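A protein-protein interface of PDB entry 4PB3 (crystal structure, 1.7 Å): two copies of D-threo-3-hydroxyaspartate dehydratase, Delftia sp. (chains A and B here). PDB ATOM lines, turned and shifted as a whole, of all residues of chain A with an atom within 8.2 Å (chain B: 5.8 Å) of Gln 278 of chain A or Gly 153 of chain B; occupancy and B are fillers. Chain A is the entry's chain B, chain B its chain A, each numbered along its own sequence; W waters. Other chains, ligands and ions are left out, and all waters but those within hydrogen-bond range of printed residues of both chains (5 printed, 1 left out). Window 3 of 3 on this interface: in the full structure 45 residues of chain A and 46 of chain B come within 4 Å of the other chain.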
ATOM      1  N   GLY A 276      15.158  27.371  -1.868  1.00  0.00           N
ATOM      2  CA  GLY A 276      14.505  26.281  -2.595  1.00  0.00           C
ATOM      3  C   GLY A 276      14.140  25.212  -1.599  1.00  0.00           C
ATOM      4  O   GLY A 276      14.284  25.431  -0.361  1.00  0.00           O
ATOM      5  N   HIS A 277      13.715  24.062  -2.142  1.00  0.00           N
ATOM      6  CA  HIS A 277      13.314  22.887  -1.340  1.00  0.00           C
ATOM      7  C   HIS A 277      13.662  21.590  -2.027  1.00  0.00           C
ATOM      8  O   HIS A 277      13.848  21.580  -3.222  1.00  0.00           O
ATOM      9  CB  HIS A 277      11.804  22.921  -1.152  1.00  0.00           C
ATOM     10  CG  HIS A 277      11.334  24.138  -0.417  1.00  0.00           C
ATOM     11  ND1 HIS A 277      10.932  25.272  -1.055  1.00  0.00           N
ATOM     12  CD2 HIS A 277      11.292  24.418   0.950  1.00  0.00           C
ATOM     13  CE1 HIS A 277      10.607  26.218  -0.151  1.00  0.00           C
ATOM     14  NE2 HIS A 277      10.828  25.704   1.080  1.00  0.00           N
ATOM     15  N   GLN A 278      13.719  20.466  -1.285  1.00  0.00           N
ATOM     16  CA  GLN A 278      13.481  19.130  -1.886  1.00  0.00           C
ATOM     17  C   GLN A 278      12.308  18.549  -1.055  1.00  0.00           C
ATOM     18  O   GLN A 278      12.539  18.065   0.054  1.00  0.00           O
ATOM     19  CB  GLN A 278      14.728  18.260  -1.765  1.00  0.00           C
ATOM     20  CG  GLN A 278      15.901  18.697  -2.697  1.00  0.00           C
ATOM     21  CD  GLN A 278      15.520  18.665  -4.185  1.00  0.00           C
ATOM     22  OE1 GLN A 278      14.457  18.241  -4.570  1.00  0.00           O
ATOM     23  NE2 GLN A 278      16.440  19.148  -5.036  1.00  0.00           N
ATOM     24  N   ALA A 279      11.086  18.745  -1.507  1.00  0.00           N
ATOM     25  CA  ALA A 279       9.932  18.609  -0.597  1.00  0.00           C
ATOM     26  C   ALA A 279       9.765  17.136  -0.213  1.00  0.00           C
ATOM     27  O   ALA A 279       9.405  16.824   0.923  1.00  0.00           O
ATOM     28  CB  ALA A 279       8.652  19.164  -1.246  1.00  0.00           C
ATOM     29  N   ASP A 280      10.120  16.228  -1.119  1.00  0.00           N
ATOM     30  CA  ASP A 280       9.995  14.823  -0.768  1.00  0.00           C
ATOM     31  C   ASP A 280      10.983  14.315   0.302  1.00  0.00           C
ATOM     32  O   ASP A 280      10.694  13.268   0.896  1.00  0.00           O
ATOM     33  CB  ASP A 280       9.978  13.932  -1.985  1.00  0.00           C
ATOM     34  CG  ASP A 280      11.326  13.776  -2.609  1.00  0.00           C
ATOM     35  OD1 ASP A 280      12.285  14.507  -2.251  1.00  0.00           O
ATOM     36  OD2 ASP A 280      11.414  12.948  -3.536  1.00  0.00           O
ATOM     37  N   LYS A 281      12.091  15.044   0.559  1.00  0.00           N
ATOM     38  CA  LYS A 281      13.043  14.732   1.618  1.00  0.00           C
ATOM     39  C   LYS A 281      12.811  15.618   2.823  1.00  0.00           C
ATOM     40  O   LYS A 281      13.510  15.489   3.777  1.00  0.00           O
ATOM     41  CB  LYS A 281      14.508  14.924   1.145  1.00  0.00           C
ATOM     42  CG  LYS A 281      14.804  13.997  -0.026  1.00  0.00           C
ATOM     43  CD  LYS A 281      16.316  13.866  -0.205  1.00  0.00           C
ATOM     44  CE  LYS A 281      16.692  14.762  -1.394  1.00  0.00           C
ATOM     45  NZ  LYS A 281      18.036  14.457  -1.949  1.00  0.00           N
ATOM     46  N   GLY A 282      11.831  16.519   2.765  1.00  0.00           N
ATOM     47  CA  GLY A 282      11.574  17.482   3.861  1.00  0.00           C
ATOM     48  C   GLY A 282      12.644  18.551   4.051  1.00  0.00           C
ATOM     49  O   GLY A 282      12.894  19.028   5.182  1.00  0.00           O
ATOM     50  N   TRP A 283      13.281  18.952   2.940  1.00  0.00           N
ATOM     51  CA  TRP A 283      14.399  19.920   3.000  1.00  0.00           C
ATOM     52  C   TRP A 283      13.971  21.271   2.580  1.00  0.00           C
ATOM     53  O   TRP A 283      13.291  21.400   1.548  1.00  0.00           O
ATOM     54  CB  TRP A 283      15.514  19.518   2.064  1.00  0.00           C
ATOM     55  CG  TRP A 283      16.332  18.304   2.383  1.00  0.00           C
ATOM     56  CD1 TRP A 283      16.204  17.400   3.452  1.00  0.00           C
ATOM     57  CD2 TRP A 283      17.432  17.798   1.543  1.00  0.00           C
ATOM     58  NE1 TRP A 283      17.182  16.407   3.357  1.00  0.00           N
ATOM     59  CE2 TRP A 283      17.950  16.585   2.214  1.00  0.00           C
ATOM     60  CE3 TRP A 283      18.015  18.212   0.359  1.00  0.00           C
ATOM     61  CZ2 TRP A 283      19.034  15.844   1.687  1.00  0.00           C
ATOM     62  CZ3 TRP A 283      19.094  17.453  -0.173  1.00  0.00           C
ATOM     63  CH2 TRP A 283      19.590  16.289   0.474  1.00  0.00           C
ATOM     64  N   ALA A 284      14.435  22.290   3.311  1.00  0.00           N
ATOM     65  CA  ALA A 284      14.465  23.692   2.780  1.00  0.00           C
ATOM     66  C   ALA A 284      15.928  24.003   2.523  1.00  0.00           C
ATOM     67  O   ALA A 284      16.813  23.506   3.210  1.00  0.00           O
ATOM     68  CB  ALA A 284      13.872  24.685   3.755  1.00  0.00           C
ATOM     69  N   ILE A 285      16.191  24.720   1.423  1.00  0.00           N
ATOM     70  CA  ILE A 285      17.580  25.069   1.117  1.00  0.00           C
ATOM     71  C   ILE A 285      17.722  26.554   1.385  1.00  0.00           C
ATOM     72  O   ILE A 285      16.813  27.339   1.020  1.00  0.00           O
ATOM     73  CB  ILE A 285      17.895  24.806  -0.386  1.00  0.00           C
ATOM     74  CG1 ILE A 285      17.417  23.412  -0.847  1.00  0.00           C
ATOM     75  CG2 ILE A 285      19.334  25.231  -0.719  1.00  0.00           C
ATOM     76  CD1 ILE A 285      18.215  22.363  -0.188  1.00  0.00           C
ATOM     77  N   HIS A 331      25.136  26.791   0.089  1.00  0.00           N
ATOM     78  CA  HIS A 331      23.810  26.258   0.272  1.00  0.00           C
ATOM     79  C   HIS A 331      23.815  25.557   1.587  1.00  0.00           C
ATOM     80  O   HIS A 331      24.651  24.684   1.780  1.00  0.00           O
ATOM     81  CB  HIS A 331      23.567  25.050  -0.745  1.00  0.00           C
ATOM     82  CG  HIS A 331      23.596  25.369  -2.210  1.00  0.00           C
ATOM     83  ND1 HIS A 331      24.719  25.587  -2.903  1.00  0.00           N
ATOM     84  CD2 HIS A 331      22.553  25.386  -3.139  1.00  0.00           C
ATOM     85  CE1 HIS A 331      24.407  25.845  -4.236  1.00  0.00           C
ATOM     86  NE2 HIS A 331      23.087  25.685  -4.385  1.00  0.00           N
ATOM     87  N   ILE A 333      21.348  23.026   4.132  1.00  0.00           N
ATOM     88  CA  ILE A 333      20.205  22.102   3.980  1.00  0.00           C
ATOM     89  C   ILE A 333      19.519  22.153   5.362  1.00  0.00           C
ATOM     90  O   ILE A 333      20.136  21.731   6.368  1.00  0.00           O
ATOM     91  CB  ILE A 333      20.633  20.624   3.758  1.00  0.00           C
ATOM     92  CG1 ILE A 333      21.575  20.409   2.546  1.00  0.00           C
ATOM     93  CG2 ILE A 333      19.411  19.723   3.635  1.00  0.00           C
ATOM     94  CD1 ILE A 333      21.070  20.947   1.291  1.00  0.00           C
ATOM     95  N   LEU A 334      18.311  22.660   5.394  1.00  0.00           N
ATOM     96  CA  LEU A 334      17.490  22.804   6.632  1.00  0.00           C
ATOM     97  C   LEU A 334      16.517  21.611   6.666  1.00  0.00           C
ATOM     98  O   LEU A 334      15.861  21.294   5.673  1.00  0.00           O
ATOM     99  CB  LEU A 334      16.733  24.138   6.614  1.00  0.00           C
ATOM    100  CG  LEU A 334      15.898  24.501   7.811  1.00  0.00           C
ATOM    101  CD1 LEU A 334      15.665  26.003   7.707  1.00  0.00           C
ATOM    102  CD2 LEU A 334      14.573  23.732   7.820  1.00  0.00           C
ATOM    103  N   ALA A 335      16.527  20.872   7.774  1.00  0.00           N
ATOM    104  CA  ALA A 335      15.670  19.694   7.830  1.00  0.00           C
ATOM    105  C   ALA A 335      15.439  19.405   9.363  1.00  0.00           C
ATOM    106  O   ALA A 335      15.946  20.079  10.230  1.00  0.00           O
ATOM    107  CB  ALA A 335      16.304  18.456   7.125  1.00  0.00           C
ATOM    108  N   ALA A 341      11.204  13.219   7.670  1.00  0.00           N
ATOM    109  CA  ALA A 341      10.891  14.167   6.573  1.00  0.00           C
ATOM    110  C   ALA A 341       9.713  15.031   7.000  1.00  0.00           C
ATOM    111  O   ALA A 341       8.581  14.524   7.068  1.00  0.00           O
ATOM    112  CB  ALA A 341      10.540  13.467   5.237  1.00  0.00           C
ATOM    113  N   GLU A 342       9.950  16.323   7.274  1.00  0.00           N
ATOM    114  CA  GLU A 342       8.825  17.224   7.468  1.00  0.00           C
ATOM    115  C   GLU A 342       7.852  17.168   6.242  1.00  0.00           C
ATOM    116  O   GLU A 342       8.303  17.391   5.100  1.00  0.00           O
ATOM    117  CB  GLU A 342       9.353  18.643   7.671  1.00  0.00           C
ATOM    118  CG  GLU A 342       8.283  19.644   8.065  1.00  0.00           C
ATOM    119  CD  GLU A 342       7.773  19.447   9.499  1.00  0.00           C
ATOM    120  OE1 GLU A 342       8.344  18.631  10.292  1.00  0.00           O
ATOM    121  OE2 GLU A 342       6.811  20.154   9.849  1.00  0.00           O
ATOM    122  N   ILE A 345       7.266  20.872   3.779  1.00  0.00           N
ATOM    123  CA  ILE A 345       8.360  21.778   4.191  1.00  0.00           C
ATOM    124  C   ILE A 345       8.212  23.197   3.565  1.00  0.00           C
ATOM    125  O   ILE A 345       8.611  24.205   4.199  1.00  0.00           O
ATOM    126  CB  ILE A 345       9.755  21.129   3.891  1.00  0.00           C
ATOM    127  CG1 ILE A 345      10.922  21.993   4.456  1.00  0.00           C
ATOM    128  CG2 ILE A 345       9.931  20.770   2.417  1.00  0.00           C
ATOM    129  CD1 ILE A 345      11.017  21.801   5.963  1.00  0.00           C
ATOM    130  N   ALA A 346       7.656  23.272   2.347  1.00  0.00           N
ATOM    131  CA  ALA A 346       7.528  24.559   1.646  1.00  0.00           C
ATOM    132  C   ALA A 346       6.481  25.486   2.294  1.00  0.00           C
ATOM    133  O   ALA A 346       6.632  26.708   2.322  1.00  0.00           O
ATOM    134  CB  ALA A 346       7.295  24.380   0.162  1.00  0.00           C
ATOM    135  N   SER B  96      20.672  28.574  -6.740  1.00  0.00           N
ATOM    136  CA  SER B  96      19.250  28.900  -6.934  1.00  0.00           C
ATOM    137  C   SER B  96      19.027  30.372  -6.636  1.00  0.00           C
ATOM    138  O   SER B  96      19.371  30.804  -5.499  1.00  0.00           O
ATOM    139  CB  SER B  96      18.342  28.162  -5.978  1.00  0.00           C
ATOM    140  OG  SER B  96      18.549  26.805  -6.103  1.00  0.00           O
ATOM    141  N   ASP B 120      15.079  26.217  -9.877  1.00  0.00           N
ATOM    142  CA  ASP B 120      14.585  24.848  -9.881  1.00  0.00           C
ATOM    143  C   ASP B 120      13.185  24.810  -9.365  1.00  0.00           C
ATOM    144  O   ASP B 120      12.698  23.730  -8.993  1.00  0.00           O
ATOM    145  CB  ASP B 120      15.510  23.935  -9.040  1.00  0.00           C
ATOM    146  CG  ASP B 120      15.425  24.218  -7.564  1.00  0.00           C
ATOM    147  OD1 ASP B 120      14.694  25.141  -7.076  1.00  0.00           O
ATOM    148  OD2 ASP B 120      16.059  23.470  -6.815  1.00  0.00           O
ATOM    149  N   GLU B 144      18.151  24.078 -13.113  1.00  0.00           N
ATOM    150  CA  GLU B 144      19.090  23.144 -12.461  1.00  0.00           C
ATOM    151  C   GLU B 144      18.357  21.804 -12.328  1.00  0.00           C
ATOM    152  O   GLU B 144      17.156  21.719 -11.925  1.00  0.00           O
ATOM    153  CB  GLU B 144      19.441  23.647 -11.071  1.00  0.00           C
ATOM    154  CG  GLU B 144      20.492  22.759 -10.397  1.00  0.00           C
ATOM    155  CD  GLU B 144      21.097  23.369  -9.138  1.00  0.00           C
ATOM    156  OE1 GLU B 144      22.150  22.845  -8.764  1.00  0.00           O
ATOM    157  OE2 GLU B 144      20.452  24.267  -8.516  1.00  0.00           O
ATOM    158  N   ILE B 145      19.102  20.737 -12.661  1.00  0.00           N
ATOM    159  CA  ILE B 145      18.574  19.384 -12.635  1.00  0.00           C
ATOM    160  C   ILE B 145      19.358  18.645 -11.504  1.00  0.00           C
ATOM    161  O   ILE B 145      20.590  18.805 -11.334  1.00  0.00           O
ATOM    162  CB  ILE B 145      18.897  18.679 -13.972  1.00  0.00           C
ATOM    163  CG1 ILE B 145      18.446  19.546 -15.131  1.00  0.00           C
ATOM    164  CG2 ILE B 145      18.300  17.229 -14.071  1.00  0.00           C
ATOM    165  CD1 ILE B 145      16.945  19.787 -15.245  1.00  0.00           C
ATOM    166  N   ASP B 146      18.588  17.829 -10.780  1.00  0.00           N
ATOM    167  CA  ASP B 146      19.109  17.042  -9.690  1.00  0.00           C
ATOM    168  C   ASP B 146      19.405  15.694 -10.352  1.00  0.00           C
ATOM    169  O   ASP B 146      18.471  14.943 -10.649  1.00  0.00           O
ATOM    170  CB  ASP B 146      18.007  16.902  -8.634  1.00  0.00           C
ATOM    171  CG  ASP B 146      18.428  15.952  -7.489  1.00  0.00           C
ATOM    172  OD1 ASP B 146      19.581  15.538  -7.484  1.00  0.00           O
ATOM    173  OD2 ASP B 146      17.652  15.731  -6.558  1.00  0.00           O
ATOM    174  N   ARG B 151      21.768  17.901  -3.797  1.00  0.00           N
ATOM    175  CA  ARG B 151      21.551  19.325  -3.358  1.00  0.00           C
ATOM    176  C   ARG B 151      20.300  19.877  -4.048  1.00  0.00           C
ATOM    177  O   ARG B 151      19.273  19.240  -3.874  1.00  0.00           O
ATOM    178  CB  ARG B 151      22.767  20.191  -3.716  1.00  0.00           C
ATOM    179  CG  ARG B 151      23.001  21.331  -2.718  1.00  0.00           C
ATOM    180  CD  ARG B 151      24.404  21.864  -2.899  1.00  0.00           C
ATOM    181  NE  ARG B 151      24.588  22.412  -4.275  1.00  0.00           N
ATOM    182  CZ  ARG B 151      25.826  22.640  -4.759  1.00  0.00           C
ATOM    183  NH1 ARG B 151      26.911  22.243  -3.986  1.00  0.00           N
ATOM    184  NH2 ARG B 151      25.983  23.290  -5.940  1.00  0.00           N
ATOM    185  N   SER B 152      20.361  21.016  -4.786  1.00  0.00           N
ATOM    186  CA  SER B 152      19.189  21.542  -5.533  1.00  0.00           C
ATOM    187  C   SER B 152      18.918  20.862  -6.858  1.00  0.00           C
ATOM    188  O   SER B 152      19.668  19.986  -7.260  1.00  0.00           O
ATOM    189  CB  SER B 152      19.251  23.012  -5.877  1.00  0.00           C
ATOM    190  OG  SER B 152      20.025  23.708  -4.964  1.00  0.00           O
ATOM    191  N   GLY B 153      17.793  21.271  -7.463  1.00  0.00           N
ATOM    192  CA  GLY B 153      17.453  20.886  -8.802  1.00  0.00           C
ATOM    193  C   GLY B 153      16.186  20.091  -8.928  1.00  0.00           C
ATOM    194  O   GLY B 153      15.709  19.491  -7.996  1.00  0.00           O
ATOM    195  N   VAL B 154      15.666  20.096 -10.154  1.00  0.00           N
ATOM    196  CA  VAL B 154      14.484  19.368 -10.552  1.00  0.00           C
ATOM    197  C   VAL B 154      14.925  17.936 -10.794  1.00  0.00           C
ATOM    198  O   VAL B 154      15.903  17.732 -11.497  1.00  0.00           O
ATOM    199  CB  VAL B 154      13.978  19.963 -11.886  1.00  0.00           C
ATOM    200  CG1 VAL B 154      12.813  19.163 -12.465  1.00  0.00           C
ATOM    201  CG2 VAL B 154      13.587  21.427 -11.702  1.00  0.00           C
ATOM    202  N   GLY B 155      14.149  16.966 -10.313  1.00  0.00           N
ATOM    203  CA  GLY B 155      14.535  15.557 -10.485  1.00  0.00           C
ATOM    204  C   GLY B 155      14.637  15.305 -11.995  1.00  0.00           C
ATOM    205  O   GLY B 155      13.836  15.792 -12.775  1.00  0.00           O
HETATM  206  O   HOH W   1      13.007  24.469  -4.982  1.00  0.00           O
HETATM  207  O   HOH W   2      23.938  24.779  -7.460  1.00  0.00           O
HETATM  208  O   HOH W   3      21.386  25.735  -6.390  1.00  0.00           O
HETATM  209  O   HOH W   4      16.072  22.968  -4.199  1.00  0.00           O
HETATM  210  O   HOH W   5      18.487  16.502  -3.796  1.00  0.00           O
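The side-chain amide nitrogen of Gln 278 of chain A is in hydrogen-bond range of the backbone carbonyl oxygen of Arg 151 of chain B, 3.1 Å away. A ring nitrogen (ND1) of His 331 of chain A lies close to the guanidinium group (NE) of Arg 151 of chain B (3.5 Å). NE2 of Gln 278 of chain A lies within hydrogen-bond range of O of Gly 153 of chain B (3.1 Å).
Among the printed residues, pairs that only touch across the chains: Gln 278 of chain A with Asp 146 of chain B, Gln 278 of chain A with Ser 152 of chain B and His 331 of chain A with Ser 152 of chain B.
The backbone NH (N) of Gly 153 of chain B sits at hydrogen-bond distance from the side-chain carboxylate (OD2) of Asp 120 of chain B, 2.9 Å away. The backbone NH of Asp 146 of chain B is in hydrogen-bond range of the backbone carbonyl oxygen of Val 154 of chain B (2.8 Å). N of Gln 278 of chain A sits at hydrogen-bond distance from O of Trp 283 of chain A, 3.0 Å away.
Water W3 lies within hydrogen-bond range of NE2 of His 331 of chain A (2.6 Å), OE2 of Glu 144 of chain B (2.7 Å), OG of Ser 152 of chain B (2.8 Å) and N of Ser 96 of chain B (2.9 Å). Water W4 lies within hydrogen-bond range of the side-chain carboxylate (OD2) of Asp 120 of chain B and the backbone carbonyl oxygen (O) of His 277 of chain A. Water W1 bridges the side-chain carboxylate (OD1) of Asp 120 of chain B and the backbone NH (N) of His 277 of chain A. Water W5 lies within hydrogen-bond range of the side-chain amino group of Lys 281 of chain A (2.8 Å), the backbone carbonyl oxygen of Arg 151 of chain B (2.8 Å) and the side-chain carboxylate of Asp 146 of chain B (3.0 Å). Water W2 lies within hydrogen-bond range of OE1 of Glu 144 of chain B, NH2 of Arg 151 of chain B and NE2 of His 331 of chain A.
No position is printed for both chains. Of the 6 pairs that touch across the chains among the printed residues, none has its exchanged pair printed and touching as well.
Of the 10 printed residues of chain B, 4 touch a printed residue of chain A. Hydrophobic or aromatic side chains of chain A within 4 Å of the printed part of chain B: His 331. Among the printed residues, no Asp or Glu carboxylate lies within 4 Å of a Lys or Arg side-chain nitrogen of the other chain.
Of the printed residues of chain B, Gln 278 of chain A touches Asp 146 (3.9 Å), Arg 151 (3.1 Å), Ser 152 (3.5 Å) and Gly 153 (3.1 Å). Gly 153 of chain B touches one residue of chain A. Ser 152 of chain B touches just these residues of chain A: Gln 278 and His 331. Of the printed residues of chain B, His 331 of chain A touches Arg 151 (3.4 Å) and Ser 152 (3.5 Å). Of the printed residues of chain A, Asp 146 of chain B touches Gln 278. Printed residues of chain A within 4 Å of Arg 151 of chain B: Gln 278 and His 331.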
